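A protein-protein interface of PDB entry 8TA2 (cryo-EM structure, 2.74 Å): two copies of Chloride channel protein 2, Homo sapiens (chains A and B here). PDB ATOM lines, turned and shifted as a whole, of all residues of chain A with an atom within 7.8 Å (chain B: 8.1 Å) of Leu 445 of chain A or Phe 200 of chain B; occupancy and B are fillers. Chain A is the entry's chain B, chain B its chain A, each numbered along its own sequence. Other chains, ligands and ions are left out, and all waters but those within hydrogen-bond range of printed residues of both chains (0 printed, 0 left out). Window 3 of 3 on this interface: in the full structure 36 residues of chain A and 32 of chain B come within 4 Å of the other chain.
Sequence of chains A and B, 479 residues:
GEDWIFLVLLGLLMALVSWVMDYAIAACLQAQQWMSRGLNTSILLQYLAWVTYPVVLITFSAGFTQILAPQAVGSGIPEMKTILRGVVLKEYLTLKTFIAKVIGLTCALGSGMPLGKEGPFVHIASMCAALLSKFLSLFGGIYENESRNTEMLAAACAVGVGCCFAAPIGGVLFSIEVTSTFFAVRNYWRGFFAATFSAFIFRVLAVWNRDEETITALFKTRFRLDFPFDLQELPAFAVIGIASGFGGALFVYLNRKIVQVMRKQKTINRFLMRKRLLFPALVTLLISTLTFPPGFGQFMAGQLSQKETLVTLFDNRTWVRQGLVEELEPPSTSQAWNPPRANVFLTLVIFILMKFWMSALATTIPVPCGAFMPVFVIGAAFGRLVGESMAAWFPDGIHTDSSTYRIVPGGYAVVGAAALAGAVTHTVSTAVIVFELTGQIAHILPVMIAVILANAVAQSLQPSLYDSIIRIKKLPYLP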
ATOM      1  N   PHE A 229      13.896  -0.142  -1.374  1.00  0.00           N
ATOM      2  CA  PHE A 229      14.214  -1.503  -0.945  1.00  0.00           C
ATOM      3  C   PHE A 229      15.669  -1.849  -1.308  1.00  0.00           C
ATOM      4  O   PHE A 229      16.301  -1.139  -2.089  1.00  0.00           O
ATOM      5  CB  PHE A 229      13.221  -2.516  -1.551  1.00  0.00           C
ATOM      6  CG  PHE A 229      13.368  -2.774  -3.040  1.00  0.00           C
ATOM      7  CD1 PHE A 229      12.698  -1.961  -3.972  1.00  0.00           C
ATOM      8  CD2 PHE A 229      14.195  -3.818  -3.497  1.00  0.00           C
ATOM      9  CE1 PHE A 229      12.893  -2.159  -5.348  1.00  0.00           C
ATOM     10  CE2 PHE A 229      14.388  -4.016  -4.873  1.00  0.00           C
ATOM     11  CZ  PHE A 229      13.746  -3.179  -5.797  1.00  0.00           C
ATOM     12  N   LEU A 231      18.617  -5.193  -2.348  1.00  0.00           N
ATOM     13  CA  LEU A 231      18.775  -6.565  -2.856  1.00  0.00           C
ATOM     14  C   LEU A 231      18.852  -7.610  -1.732  1.00  0.00           C
ATOM     15  O   LEU A 231      18.513  -8.769  -1.954  1.00  0.00           O
ATOM     16  CB  LEU A 231      20.035  -6.670  -3.738  1.00  0.00           C
ATOM     17  CG  LEU A 231      19.818  -6.358  -5.225  1.00  0.00           C
ATOM     18  CD1 LEU A 231      19.415  -4.909  -5.488  1.00  0.00           C
ATOM     19  CD2 LEU A 231      21.111  -6.651  -5.976  1.00  0.00           C
ATOM     20  N   LEU A 234      15.108  -8.714  -1.352  1.00  0.00           N
ATOM     21  CA  LEU A 234      14.439  -9.470  -2.424  1.00  0.00           C
ATOM     22  C   LEU A 234      14.030 -10.906  -2.027  1.00  0.00           C
ATOM     23  O   LEU A 234      12.959 -11.327  -2.461  1.00  0.00           O
ATOM     24  CB  LEU A 234      15.247  -9.457  -3.735  1.00  0.00           C
ATOM     25  CG  LEU A 234      15.245  -8.111  -4.484  1.00  0.00           C
ATOM     26  CD1 LEU A 234      16.111  -8.229  -5.731  1.00  0.00           C
ATOM     27  CD2 LEU A 234      13.848  -7.677  -4.927  1.00  0.00           C
ATOM     28  N   PRO A 235      14.752 -11.652  -1.170  1.00  0.00           N
ATOM     29  CA  PRO A 235      14.293 -12.957  -0.684  1.00  0.00           C
ATOM     30  C   PRO A 235      12.990 -12.923   0.134  1.00  0.00           C
ATOM     31  O   PRO A 235      12.296 -13.935   0.206  1.00  0.00           O
ATOM     32  CB  PRO A 235      15.450 -13.515   0.149  1.00  0.00           C
ATOM     33  CG  PRO A 235      16.671 -12.847  -0.464  1.00  0.00           C
ATOM     34  CD  PRO A 235      16.143 -11.463  -0.803  1.00  0.00           C
ATOM     35  N   PHE A 237      10.308 -10.534  -0.520  1.00  0.00           N
ATOM     36  CA  PHE A 237       9.303 -10.384  -1.581  1.00  0.00           C
ATOM     37  C   PHE A 237       9.087 -11.670  -2.403  1.00  0.00           C
ATOM     38  O   PHE A 237       7.979 -11.945  -2.851  1.00  0.00           O
ATOM     39  CB  PHE A 237       9.698  -9.230  -2.497  1.00  0.00           C
ATOM     40  CG  PHE A 237       9.804  -7.871  -1.832  1.00  0.00           C
ATOM     41  CD1 PHE A 237       8.648  -7.206  -1.396  1.00  0.00           C
ATOM     42  CD2 PHE A 237      11.047  -7.219  -1.736  1.00  0.00           C
ATOM     43  CE1 PHE A 237       8.728  -5.883  -0.933  1.00  0.00           C
ATOM     44  CE2 PHE A 237      11.130  -5.907  -1.247  1.00  0.00           C
ATOM     45  CZ  PHE A 237       9.967  -5.231  -0.862  1.00  0.00           C
ATOM     46  N   VAL A 415       2.829  -5.678  -2.726  1.00  0.00           N
ATOM     47  CA  VAL A 415       3.325  -6.930  -3.307  1.00  0.00           C
ATOM     48  C   VAL A 415       2.447  -8.122  -2.916  1.00  0.00           C
ATOM     49  O   VAL A 415       2.148  -8.962  -3.757  1.00  0.00           O
ATOM     50  CB  VAL A 415       4.801  -7.141  -2.915  1.00  0.00           C
ATOM     51  CG1 VAL A 415       5.374  -8.455  -3.428  1.00  0.00           C
ATOM     52  CG2 VAL A 415       5.673  -6.032  -3.496  1.00  0.00           C
ATOM     53  N   PHE A 435       0.360  -0.722 -10.200  1.00  0.00           N
ATOM     54  CA  PHE A 435       1.068   0.509 -10.550  1.00  0.00           C
ATOM     55  C   PHE A 435       0.110   1.653 -10.877  1.00  0.00           C
ATOM     56  O   PHE A 435       0.241   2.739 -10.323  1.00  0.00           O
ATOM     57  CB  PHE A 435       2.030   0.255 -11.711  1.00  0.00           C
ATOM     58  CG  PHE A 435       3.000  -0.892 -11.511  1.00  0.00           C
ATOM     59  CD1 PHE A 435       3.530  -1.174 -10.235  1.00  0.00           C
ATOM     60  CD2 PHE A 435       3.361  -1.699 -12.602  1.00  0.00           C
ATOM     61  CE1 PHE A 435       4.346  -2.298 -10.039  1.00  0.00           C
ATOM     62  CE2 PHE A 435       4.184  -2.819 -12.403  1.00  0.00           C
ATOM     63  CZ  PHE A 435       4.647  -3.138 -11.118  1.00  0.00           C
ATOM     64  N   ILE A 441       5.705   3.342  -9.322  1.00  0.00           N
ATOM     65  CA  ILE A 441       6.395   2.251 -10.040  1.00  0.00           C
ATOM     66  C   ILE A 441       7.654   1.751  -9.301  1.00  0.00           C
ATOM     67  O   ILE A 441       8.211   0.719  -9.655  1.00  0.00           O
ATOM     68  CB  ILE A 441       6.620   2.697 -11.515  1.00  0.00           C
ATOM     69  CG1 ILE A 441       5.294   2.486 -12.275  1.00  0.00           C
ATOM     70  CG2 ILE A 441       7.769   1.999 -12.260  1.00  0.00           C
ATOM     71  CD1 ILE A 441       5.253   3.042 -13.690  1.00  0.00           C
ATOM     72  N   ALA A 442       8.084   2.398  -8.218  1.00  0.00           N
ATOM     73  CA  ALA A 442       9.332   2.091  -7.515  1.00  0.00           C
ATOM     74  C   ALA A 442       9.491   0.639  -7.012  1.00  0.00           C
ATOM     75  O   ALA A 442      10.613   0.158  -6.887  1.00  0.00           O
ATOM     76  CB  ALA A 442       9.459   3.091  -6.366  1.00  0.00           C
ATOM     77  N   HIS A 443       8.393  -0.082  -6.756  1.00  0.00           N
ATOM     78  CA  HIS A 443       8.360  -1.493  -6.320  1.00  0.00           C
ATOM     79  C   HIS A 443       8.144  -2.496  -7.465  1.00  0.00           C
ATOM     80  O   HIS A 443       7.813  -3.649  -7.216  1.00  0.00           O
ATOM     81  CB  HIS A 443       7.333  -1.663  -5.183  1.00  0.00           C
ATOM     82  CG  HIS A 443       7.777  -1.103  -3.855  1.00  0.00           C
ATOM     83  ND1 HIS A 443       8.442  -1.826  -2.863  1.00  0.00           N
ATOM     84  CD2 HIS A 443       7.617   0.182  -3.432  1.00  0.00           C
ATOM     85  CE1 HIS A 443       8.653  -0.964  -1.860  1.00  0.00           C
ATOM     86  NE2 HIS A 443       8.170   0.247  -2.177  1.00  0.00           N
ATOM     87  N   ILE A 444       8.341  -2.099  -8.724  1.00  0.00           N
ATOM     88  CA  ILE A 444       8.093  -2.921  -9.920  1.00  0.00           C
ATOM     89  C   ILE A 444       8.766  -4.297  -9.931  1.00  0.00           C
ATOM     90  O   ILE A 444       8.078  -5.290 -10.140  1.00  0.00           O
ATOM     91  CB  ILE A 444       8.398  -2.113 -11.194  1.00  0.00           C
ATOM     92  CG1 ILE A 444       8.072  -2.934 -12.453  1.00  0.00           C
ATOM     93  CG2 ILE A 444       9.848  -1.593 -11.266  1.00  0.00           C
ATOM     94  CD1 ILE A 444       7.856  -2.073 -13.691  1.00  0.00           C
ATOM     95  N   LEU A 445      10.070  -4.402  -9.670  1.00  0.00           N
ATOM     96  CA  LEU A 445      10.761  -5.694  -9.638  1.00  0.00           C
ATOM     97  C   LEU A 445      10.255  -6.620  -8.508  1.00  0.00           C
ATOM     98  O   LEU A 445       9.916  -7.761  -8.817  1.00  0.00           O
ATOM     99  CB  LEU A 445      12.290  -5.470  -9.661  1.00  0.00           C
ATOM    100  CG  LEU A 445      13.119  -6.766  -9.632  1.00  0.00           C
ATOM    101  CD1 LEU A 445      13.019  -7.534 -10.943  1.00  0.00           C
ATOM    102  CD2 LEU A 445      14.587  -6.465  -9.386  1.00  0.00           C
ATOM    103  N   PRO A 446      10.103  -6.167  -7.241  1.00  0.00           N
ATOM    104  CA  PRO A 446       9.414  -6.920  -6.192  1.00  0.00           C
ATOM    105  C   PRO A 446       8.028  -7.457  -6.586  1.00  0.00           C
ATOM    106  O   PRO A 446       7.770  -8.651  -6.427  1.00  0.00           O
ATOM    107  CB  PRO A 446       9.299  -5.944  -5.023  1.00  0.00           C
ATOM    108  CG  PRO A 446      10.530  -5.067  -5.154  1.00  0.00           C
ATOM    109  CD  PRO A 446      10.722  -4.980  -6.659  1.00  0.00           C
ATOM    110  N   VAL A 447       7.149  -6.608  -7.135  1.00  0.00           N
ATOM    111  CA  VAL A 447       5.811  -6.999  -7.593  1.00  0.00           C
ATOM    112  C   VAL A 447       5.892  -8.109  -8.637  1.00  0.00           C
ATOM    113  O   VAL A 447       5.241  -9.136  -8.487  1.00  0.00           O
ATOM    114  CB  VAL A 447       5.053  -5.773  -8.133  1.00  0.00           C
ATOM    115  CG1 VAL A 447       3.809  -6.122  -8.948  1.00  0.00           C
ATOM    116  CG2 VAL A 447       4.600  -4.872  -6.985  1.00  0.00           C
ATOM    117  N   MET A 448       6.707  -7.949  -9.679  1.00  0.00           N
ATOM    118  CA  MET A 448       6.805  -8.915 -10.766  1.00  0.00           C
ATOM    119  C   MET A 448       7.401 -10.255 -10.337  1.00  0.00           C
ATOM    120  O   MET A 448       6.944 -11.290 -10.809  1.00  0.00           O
ATOM    121  CB  MET A 448       7.602  -8.307 -11.917  1.00  0.00           C
ATOM    122  CG  MET A 448       6.841  -7.145 -12.561  1.00  0.00           C
ATOM    123  SD  MET A 448       7.709  -6.331 -13.918  1.00  0.00           S
ATOM    124  CE  MET A 448       7.585  -7.589 -15.208  1.00  0.00           C
ATOM    125  N   ILE A 449       8.358 -10.276  -9.408  1.00  0.00           N
ATOM    126  CA  ILE A 449       8.865 -11.527  -8.834  1.00  0.00           C
ATOM    127  C   ILE A 449       7.760 -12.240  -8.051  1.00  0.00           C
ATOM    128  O   ILE A 449       7.519 -13.426  -8.255  1.00  0.00           O
ATOM    129  CB  ILE A 449      10.112 -11.257  -7.963  1.00  0.00           C
ATOM    130  CG1 ILE A 449      11.303 -10.856  -8.850  1.00  0.00           C
ATOM    131  CG2 ILE A 449      10.474 -12.482  -7.104  1.00  0.00           C
ATOM    132  CD1 ILE A 449      12.487 -10.274  -8.069  1.00  0.00           C
ATOM    133  N   ALA A 450       7.038 -11.536  -7.182  1.00  0.00           N
ATOM    134  CA  ALA A 450       5.989 -12.151  -6.388  1.00  0.00           C
ATOM    135  C   ALA A 450       4.848 -12.680  -7.259  1.00  0.00           C
ATOM    136  O   ALA A 450       4.447 -13.829  -7.104  1.00  0.00           O
ATOM    137  CB  ALA A 450       5.486 -11.143  -5.364  1.00  0.00           C
ATOM    138  N   VAL A 451       4.354 -11.874  -8.201  1.00  0.00           N
ATOM    139  CA  VAL A 451       3.265 -12.241  -9.114  1.00  0.00           C
ATOM    140  C   VAL A 451       3.608 -13.458  -9.974  1.00  0.00           C
ATOM    141  O   VAL A 451       2.774 -14.353 -10.097  1.00  0.00           O
ATOM    142  CB  VAL A 451       2.846 -11.022  -9.951  1.00  0.00           C
ATOM    143  CG1 VAL A 451       1.948 -11.348 -11.141  1.00  0.00           C
ATOM    144  CG2 VAL A 451       2.087 -10.021  -9.077  1.00  0.00           C
ATOM    145  N   ILE A 452       4.817 -13.566 -10.525  1.00  0.00           N
ATOM    146  CA  ILE A 452       5.192 -14.734 -11.325  1.00  0.00           C
ATOM    147  C   ILE A 452       5.451 -15.974 -10.463  1.00  0.00           C
ATOM    148  O   ILE A 452       5.117 -17.072 -10.889  1.00  0.00           O
ATOM    149  CB  ILE A 452       6.331 -14.396 -12.316  1.00  0.00           C
ATOM    150  CG1 ILE A 452       6.344 -15.341 -13.531  1.00  0.00           C
ATOM    151  CG2 ILE A 452       7.728 -14.448 -11.685  1.00  0.00           C
ATOM    152  CD1 ILE A 452       5.116 -15.247 -14.444  1.00  0.00           C
ATOM    153  N   GLY B  11      16.862 -15.072 -20.428  1.00  0.00           N
ATOM    154  CA  GLY B  11      16.829 -13.813 -19.684  1.00  0.00           C
ATOM    155  C   GLY B  11      18.205 -13.362 -19.180  1.00  0.00           C
ATOM    156  O   GLY B  11      18.481 -12.165 -19.145  1.00  0.00           O
ATOM    157  N   LEU B  12      19.077 -14.313 -18.830  1.00  0.00           N
ATOM    158  CA  LEU B  12      20.460 -14.091 -18.407  1.00  0.00           C
ATOM    159  C   LEU B  12      21.361 -13.686 -19.581  1.00  0.00           C
ATOM    160  O   LEU B  12      22.000 -12.639 -19.528  1.00  0.00           O
ATOM    161  CB  LEU B  12      20.960 -15.382 -17.735  1.00  0.00           C
ATOM    162  CG  LEU B  12      22.431 -15.365 -17.290  1.00  0.00           C
ATOM    163  CD1 LEU B  12      22.687 -14.321 -16.211  1.00  0.00           C
ATOM    164  CD2 LEU B  12      22.830 -16.729 -16.738  1.00  0.00           C
ATOM    165  N   ALA B  15      20.598 -10.214 -21.291  1.00  0.00           N
ATOM    166  CA  ALA B  15      20.987  -9.133 -20.383  1.00  0.00           C
ATOM    167  C   ALA B  15      22.514  -8.940 -20.321  1.00  0.00           C
ATOM    168  O   ALA B  15      22.994  -7.814 -20.415  1.00  0.00           O
ATOM    169  CB  ALA B  15      20.389  -9.409 -19.004  1.00  0.00           C
ATOM    170  N   PRO B 168      10.401  -3.814 -18.636  1.00  0.00           N
ATOM    171  CA  PRO B 168      10.061  -5.234 -18.647  1.00  0.00           C
ATOM    172  C   PRO B 168       8.628  -5.589 -19.047  1.00  0.00           C
ATOM    173  O   PRO B 168       8.435  -6.667 -19.600  1.00  0.00           O
ATOM    174  CB  PRO B 168      10.353  -5.736 -17.234  1.00  0.00           C
ATOM    175  CG  PRO B 168      11.468  -4.814 -16.779  1.00  0.00           C
ATOM    176  CD  PRO B 168      11.036  -3.484 -17.368  1.00  0.00           C
ATOM    177  N   PHE B 192       6.479 -12.084 -19.971  1.00  0.00           N
ATOM    178  CA  PHE B 192       6.552 -11.508 -18.626  1.00  0.00           C
ATOM    179  C   PHE B 192       7.553 -12.261 -17.735  1.00  0.00           C
ATOM    180  O   PHE B 192       8.358 -11.636 -17.054  1.00  0.00           O
ATOM    181  CB  PHE B 192       5.123 -11.496 -18.054  1.00  0.00           C
ATOM    182  CG  PHE B 192       4.905 -10.745 -16.752  1.00  0.00           C
ATOM    183  CD1 PHE B 192       5.348 -11.286 -15.531  1.00  0.00           C
ATOM    184  CD2 PHE B 192       4.189  -9.536 -16.750  1.00  0.00           C
ATOM    185  CE1 PHE B 192       5.086 -10.620 -14.325  1.00  0.00           C
ATOM    186  CE2 PHE B 192       3.917  -8.874 -15.543  1.00  0.00           C
ATOM    187  CZ  PHE B 192       4.366  -9.417 -14.331  1.00  0.00           C
ATOM    188  N   ALA B 194      10.326 -14.137 -18.667  1.00  0.00           N
ATOM    189  CA  ALA B 194      11.693 -13.939 -19.141  1.00  0.00           C
ATOM    190  C   ALA B 194      12.150 -12.476 -19.047  1.00  0.00           C
ATOM    191  O   ALA B 194      13.281 -12.220 -18.650  1.00  0.00           O
ATOM    192  CB  ALA B 194      11.777 -14.489 -20.558  1.00  0.00           C
ATOM    193  N   ALA B 195      11.281 -11.499 -19.306  1.00  0.00           N
ATOM    194  CA  ALA B 195      11.584 -10.096 -19.058  1.00  0.00           C
ATOM    195  C   ALA B 195      11.818  -9.766 -17.570  1.00  0.00           C
ATOM    196  O   ALA B 195      12.536  -8.817 -17.262  1.00  0.00           O
ATOM    197  CB  ALA B 195      10.459  -9.248 -19.642  1.00  0.00           C
ATOM    198  N   THR B 196      11.277 -10.551 -16.630  1.00  0.00           N
ATOM    199  CA  THR B 196      11.541 -10.377 -15.191  1.00  0.00           C
ATOM    200  C   THR B 196      12.955 -10.811 -14.822  1.00  0.00           C
ATOM    201  O   THR B 196      13.649 -10.075 -14.127  1.00  0.00           O
ATOM    202  CB  THR B 196      10.516 -11.129 -14.328  1.00  0.00           C
ATOM    203  OG1 THR B 196       9.238 -10.627 -14.597  1.00  0.00           O
ATOM    204  CG2 THR B 196      10.722 -10.978 -12.821  1.00  0.00           C
ATOM    205  N   PHE B 197      13.436 -11.963 -15.296  1.00  0.00           N
ATOM    206  CA  PHE B 197      14.789 -12.420 -14.967  1.00  0.00           C
ATOM    207  C   PHE B 197      15.885 -11.514 -15.558  1.00  0.00           C
ATOM    208  O   PHE B 197      16.913 -11.303 -14.926  1.00  0.00           O
ATOM    209  CB  PHE B 197      14.980 -13.879 -15.377  1.00  0.00           C
ATOM    210  CG  PHE B 197      16.136 -14.528 -14.643  1.00  0.00           C
ATOM    211  CD1 PHE B 197      15.921 -15.110 -13.382  1.00  0.00           C
ATOM    212  CD2 PHE B 197      17.437 -14.498 -15.177  1.00  0.00           C
ATOM    213  CE1 PHE B 197      16.996 -15.656 -12.660  1.00  0.00           C
ATOM    214  CE2 PHE B 197      18.514 -15.039 -14.452  1.00  0.00           C
ATOM    215  CZ  PHE B 197      18.293 -15.618 -13.194  1.00  0.00           C
ATOM    216  N   SER B 198      15.659 -10.875 -16.711  1.00  0.00           N
ATOM    217  CA  SER B 198      16.560  -9.832 -17.218  1.00  0.00           C
ATOM    218  C   SER B 198      16.585  -8.585 -16.332  1.00  0.00           C
ATOM    219  O   SER B 198      17.656  -8.054 -16.062  1.00  0.00           O
ATOM    220  CB  SER B 198      16.202  -9.416 -18.645  1.00  0.00           C
ATOM    221  OG  SER B 198      16.275 -10.528 -19.503  1.00  0.00           O
ATOM    222  N   ALA B 199      15.438  -8.117 -15.838  1.00  0.00           N
ATOM    223  CA  ALA B 199      15.354  -6.951 -14.951  1.00  0.00           C
ATOM    224  C   ALA B 199      16.046  -7.164 -13.591  1.00  0.00           C
ATOM    225  O   ALA B 199      16.630  -6.236 -13.040  1.00  0.00           O
ATOM    226  CB  ALA B 199      13.880  -6.611 -14.761  1.00  0.00           C
ATOM    227  N   PHE B 200      16.041  -8.395 -13.078  1.00  0.00           N
ATOM    228  CA  PHE B 200      16.834  -8.789 -11.921  1.00  0.00           C
ATOM    229  C   PHE B 200      18.342  -8.718 -12.205  1.00  0.00           C
ATOM    230  O   PHE B 200      19.053  -7.993 -11.510  1.00  0.00           O
ATOM    231  CB  PHE B 200      16.397 -10.178 -11.460  1.00  0.00           C
ATOM    232  CG  PHE B 200      17.279 -10.791 -10.397  1.00  0.00           C
ATOM    233  CD1 PHE B 200      17.386 -10.187  -9.133  1.00  0.00           C
ATOM    234  CD2 PHE B 200      17.995 -11.970 -10.673  1.00  0.00           C
ATOM    235  CE1 PHE B 200      18.216 -10.753  -8.153  1.00  0.00           C
ATOM    236  CE2 PHE B 200      18.822 -12.537  -9.693  1.00  0.00           C
ATOM    237  CZ  PHE B 200      18.937 -11.926  -8.434  1.00  0.00           C
ATOM    238  N   ILE B 201      18.841  -9.383 -13.258  1.00  0.00           N
ATOM    239  CA  ILE B 201      20.266  -9.358 -13.627  1.00  0.00           C
ATOM    240  C   ILE B 201      20.765  -7.937 -13.910  1.00  0.00           C
ATOM    241  O   ILE B 201      21.838  -7.570 -13.449  1.00  0.00           O
ATOM    242  CB  ILE B 201      20.523 -10.311 -14.812  1.00  0.00           C
ATOM    243  CG1 ILE B 201      20.279 -11.784 -14.426  1.00  0.00           C
ATOM    244  CG2 ILE B 201      21.933 -10.151 -15.407  1.00  0.00           C
ATOM    245  CD1 ILE B 201      21.188 -12.354 -13.332  1.00  0.00           C
ATOM    246  N   PHE B 202      19.976  -7.090 -14.567  1.00  0.00           N
ATOM    247  CA  PHE B 202      20.298  -5.677 -14.770  1.00  0.00           C
ATOM    248  C   PHE B 202      20.601  -4.936 -13.456  1.00  0.00           C
ATOM    249  O   PHE B 202      21.587  -4.204 -13.396  1.00  0.00           O
ATOM    250  CB  PHE B 202      19.140  -5.031 -15.536  1.00  0.00           C
ATOM    251  CG  PHE B 202      19.232  -3.532 -15.748  1.00  0.00           C
ATOM    252  CD1 PHE B 202      18.695  -2.652 -14.789  1.00  0.00           C
ATOM    253  CD2 PHE B 202      19.796  -3.014 -16.929  1.00  0.00           C
ATOM    254  CE1 PHE B 202      18.722  -1.263 -15.008  1.00  0.00           C
ATOM    255  CE2 PHE B 202      19.813  -1.624 -17.156  1.00  0.00           C
ATOM    256  CZ  PHE B 202      19.273  -0.750 -16.195  1.00  0.00           C
ATOM    257  N   ARG B 203      19.819  -5.142 -12.381  1.00  0.00           N
ATOM    258  CA  ARG B 203      20.080  -4.530 -11.064  1.00  0.00           C
ATOM    259  C   ARG B 203      21.259  -5.151 -10.326  1.00  0.00           C
ATOM    260  O   ARG B 203      22.037  -4.410  -9.740  1.00  0.00           O
ATOM    261  CB  ARG B 203      18.825  -4.519 -10.183  1.00  0.00           C
ATOM    262  CG  ARG B 203      17.923  -3.334 -10.556  1.00  0.00           C
ATOM    263  CD  ARG B 203      16.781  -3.109  -9.559  1.00  0.00           C
ATOM    264  NE  ARG B 203      17.262  -2.662  -8.235  1.00  0.00           N
ATOM    265  CZ  ARG B 203      16.848  -1.631  -7.524  1.00  0.00           C
ATOM    266  NH1 ARG B 203      17.381  -1.371  -6.371  1.00  0.00           N
ATOM    267  NH2 ARG B 203      15.912  -0.837  -7.931  1.00  0.00           N
ATOM    268  N   VAL B 204      21.467  -6.463 -10.390  1.00  0.00           N
ATOM    269  CA  VAL B 204      22.678  -7.092  -9.839  1.00  0.00           C
ATOM    270  C   VAL B 204      23.948  -6.490 -10.451  1.00  0.00           C
ATOM    271  O   VAL B 204      24.867  -6.131  -9.717  1.00  0.00           O
ATOM    272  CB  VAL B 204      22.637  -8.617 -10.020  1.00  0.00           C
ATOM    273  CG1 VAL B 204      23.943  -9.290  -9.590  1.00  0.00           C
ATOM    274  CG2 VAL B 204      21.511  -9.226  -9.184  1.00  0.00           C
ATOM    275  N   LEU B 205      23.989  -6.289 -11.774  1.00  0.00           N
ATOM    276  CA  LEU B 205      25.105  -5.618 -12.449  1.00  0.00           C
ATOM    277  C   LEU B 205      25.205  -4.136 -12.066  1.00  0.00           C
ATOM    278  O   LEU B 205      26.304  -3.640 -11.838  1.00  0.00           O
ATOM    279  CB  LEU B 205      24.971  -5.790 -13.973  1.00  0.00           C
ATOM    280  CG  LEU B 205      25.069  -7.244 -14.468  1.00  0.00           C
ATOM    281  CD1 LEU B 205      24.750  -7.301 -15.958  1.00  0.00           C
ATOM    282  CD2 LEU B 205      26.453  -7.841 -14.254  1.00  0.00           C
ATOM    283  N   ALA B 206      24.088  -3.417 -11.936  1.00  0.00           N
ATOM    284  CA  ALA B 206      24.079  -2.016 -11.509  1.00  0.00           C
ATOM    285  C   ALA B 206      24.557  -1.802 -10.057  1.00  0.00           C
ATOM    286  O   ALA B 206      24.957  -0.697  -9.693  1.00  0.00           O
ATOM    287  CB  ALA B 206      22.678  -1.443 -11.717  1.00  0.00           C
ATOM    288  N   VAL B 207      24.559  -2.840  -9.220  1.00  0.00           N
ATOM    289  CA  VAL B 207      25.324  -2.851  -7.969  1.00  0.00           C
ATOM    290  C   VAL B 207      26.787  -3.175  -8.268  1.00  0.00           C
ATOM    291  O   VAL B 207      27.654  -2.310  -8.148  1.00  0.00           O
ATOM    292  CB  VAL B 207      24.700  -3.811  -6.936  1.00  0.00           C
ATOM    293  CG1 VAL B 207      25.579  -4.004  -5.698  1.00  0.00           C
ATOM    294  CG2 VAL B 207      23.349  -3.269  -6.468  1.00  0.00           C
ATOM    295  N   GLU B 436       7.649   3.050 -17.400  1.00  0.00           N
ATOM    296  CA  GLU B 436       8.782   2.281 -16.882  1.00  0.00           C
ATOM    297  C   GLU B 436      10.127   3.004 -17.077  1.00  0.00           C
ATOM    298  O   GLU B 436      10.918   3.068 -16.137  1.00  0.00           O
ATOM    299  CB  GLU B 436       8.810   0.897 -17.536  1.00  0.00           C
ATOM    300  CG  GLU B 436       7.582   0.059 -17.178  1.00  0.00           C
ATOM    301  CD  GLU B 436       7.647  -1.316 -17.853  1.00  0.00           C
ATOM    302  OE1 GLU B 436       7.385  -1.408 -19.067  1.00  0.00           O
ATOM    303  OE2 GLU B 436       7.963  -2.312 -17.170  1.00  0.00           O
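Printed residues of chain B within 4 Å of Phe 229 of chain A: Arg 203. Of the printed residues of chain B, Leu 445 of chain A touches Phe 200 (3.8 Å). Of the printed residues of chain B, Met 448 of chain A touches Pro 168, Phe 192 and Thr 196. Of the printed residues of chain A, Pro 168 of chain B touches Met 448. Printed residues of chain A within 4 Å of Phe 192 of chain B: Met 448 (3.8 Å). Printed residues of chain A within 4 Å of Arg 203 of chain B: Phe 229. The nearest printed residue of chain B that does not touch Leu 445 of chain A is Arg 203 of chain B (4.01 Å). The nearest residue of chain A that does not touch Phe 200 of chain B is Leu 234 of chain A (4.1 Å). The nearest printed residue of chain A that does not touch Glu 436 of chain B is Ile 441 of chain A (4.4 Å).
OG1 of Thr 196 of chain B is in hydrogen-bond range of O of Phe 192 of chain B (2.8 Å).
No position is printed for both chains.
Among the printed residues, pairs that only touch across the chains: Ile 444 of chain A with Glu 436 of chain B (3.5 Å), Met 448 of chain A with Thr 196 of chain B (3.5 Å), Met 448 of chain A with Phe 192 of chain B (3.8 Å), Leu 445 of chain A with Phe 200 of chain B (3.8 Å), Phe 229 of chain A with Arg 203 of chain B (3.8 Å) and Met 448 of chain A with Pro 168 of chain B (3.9 Å).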
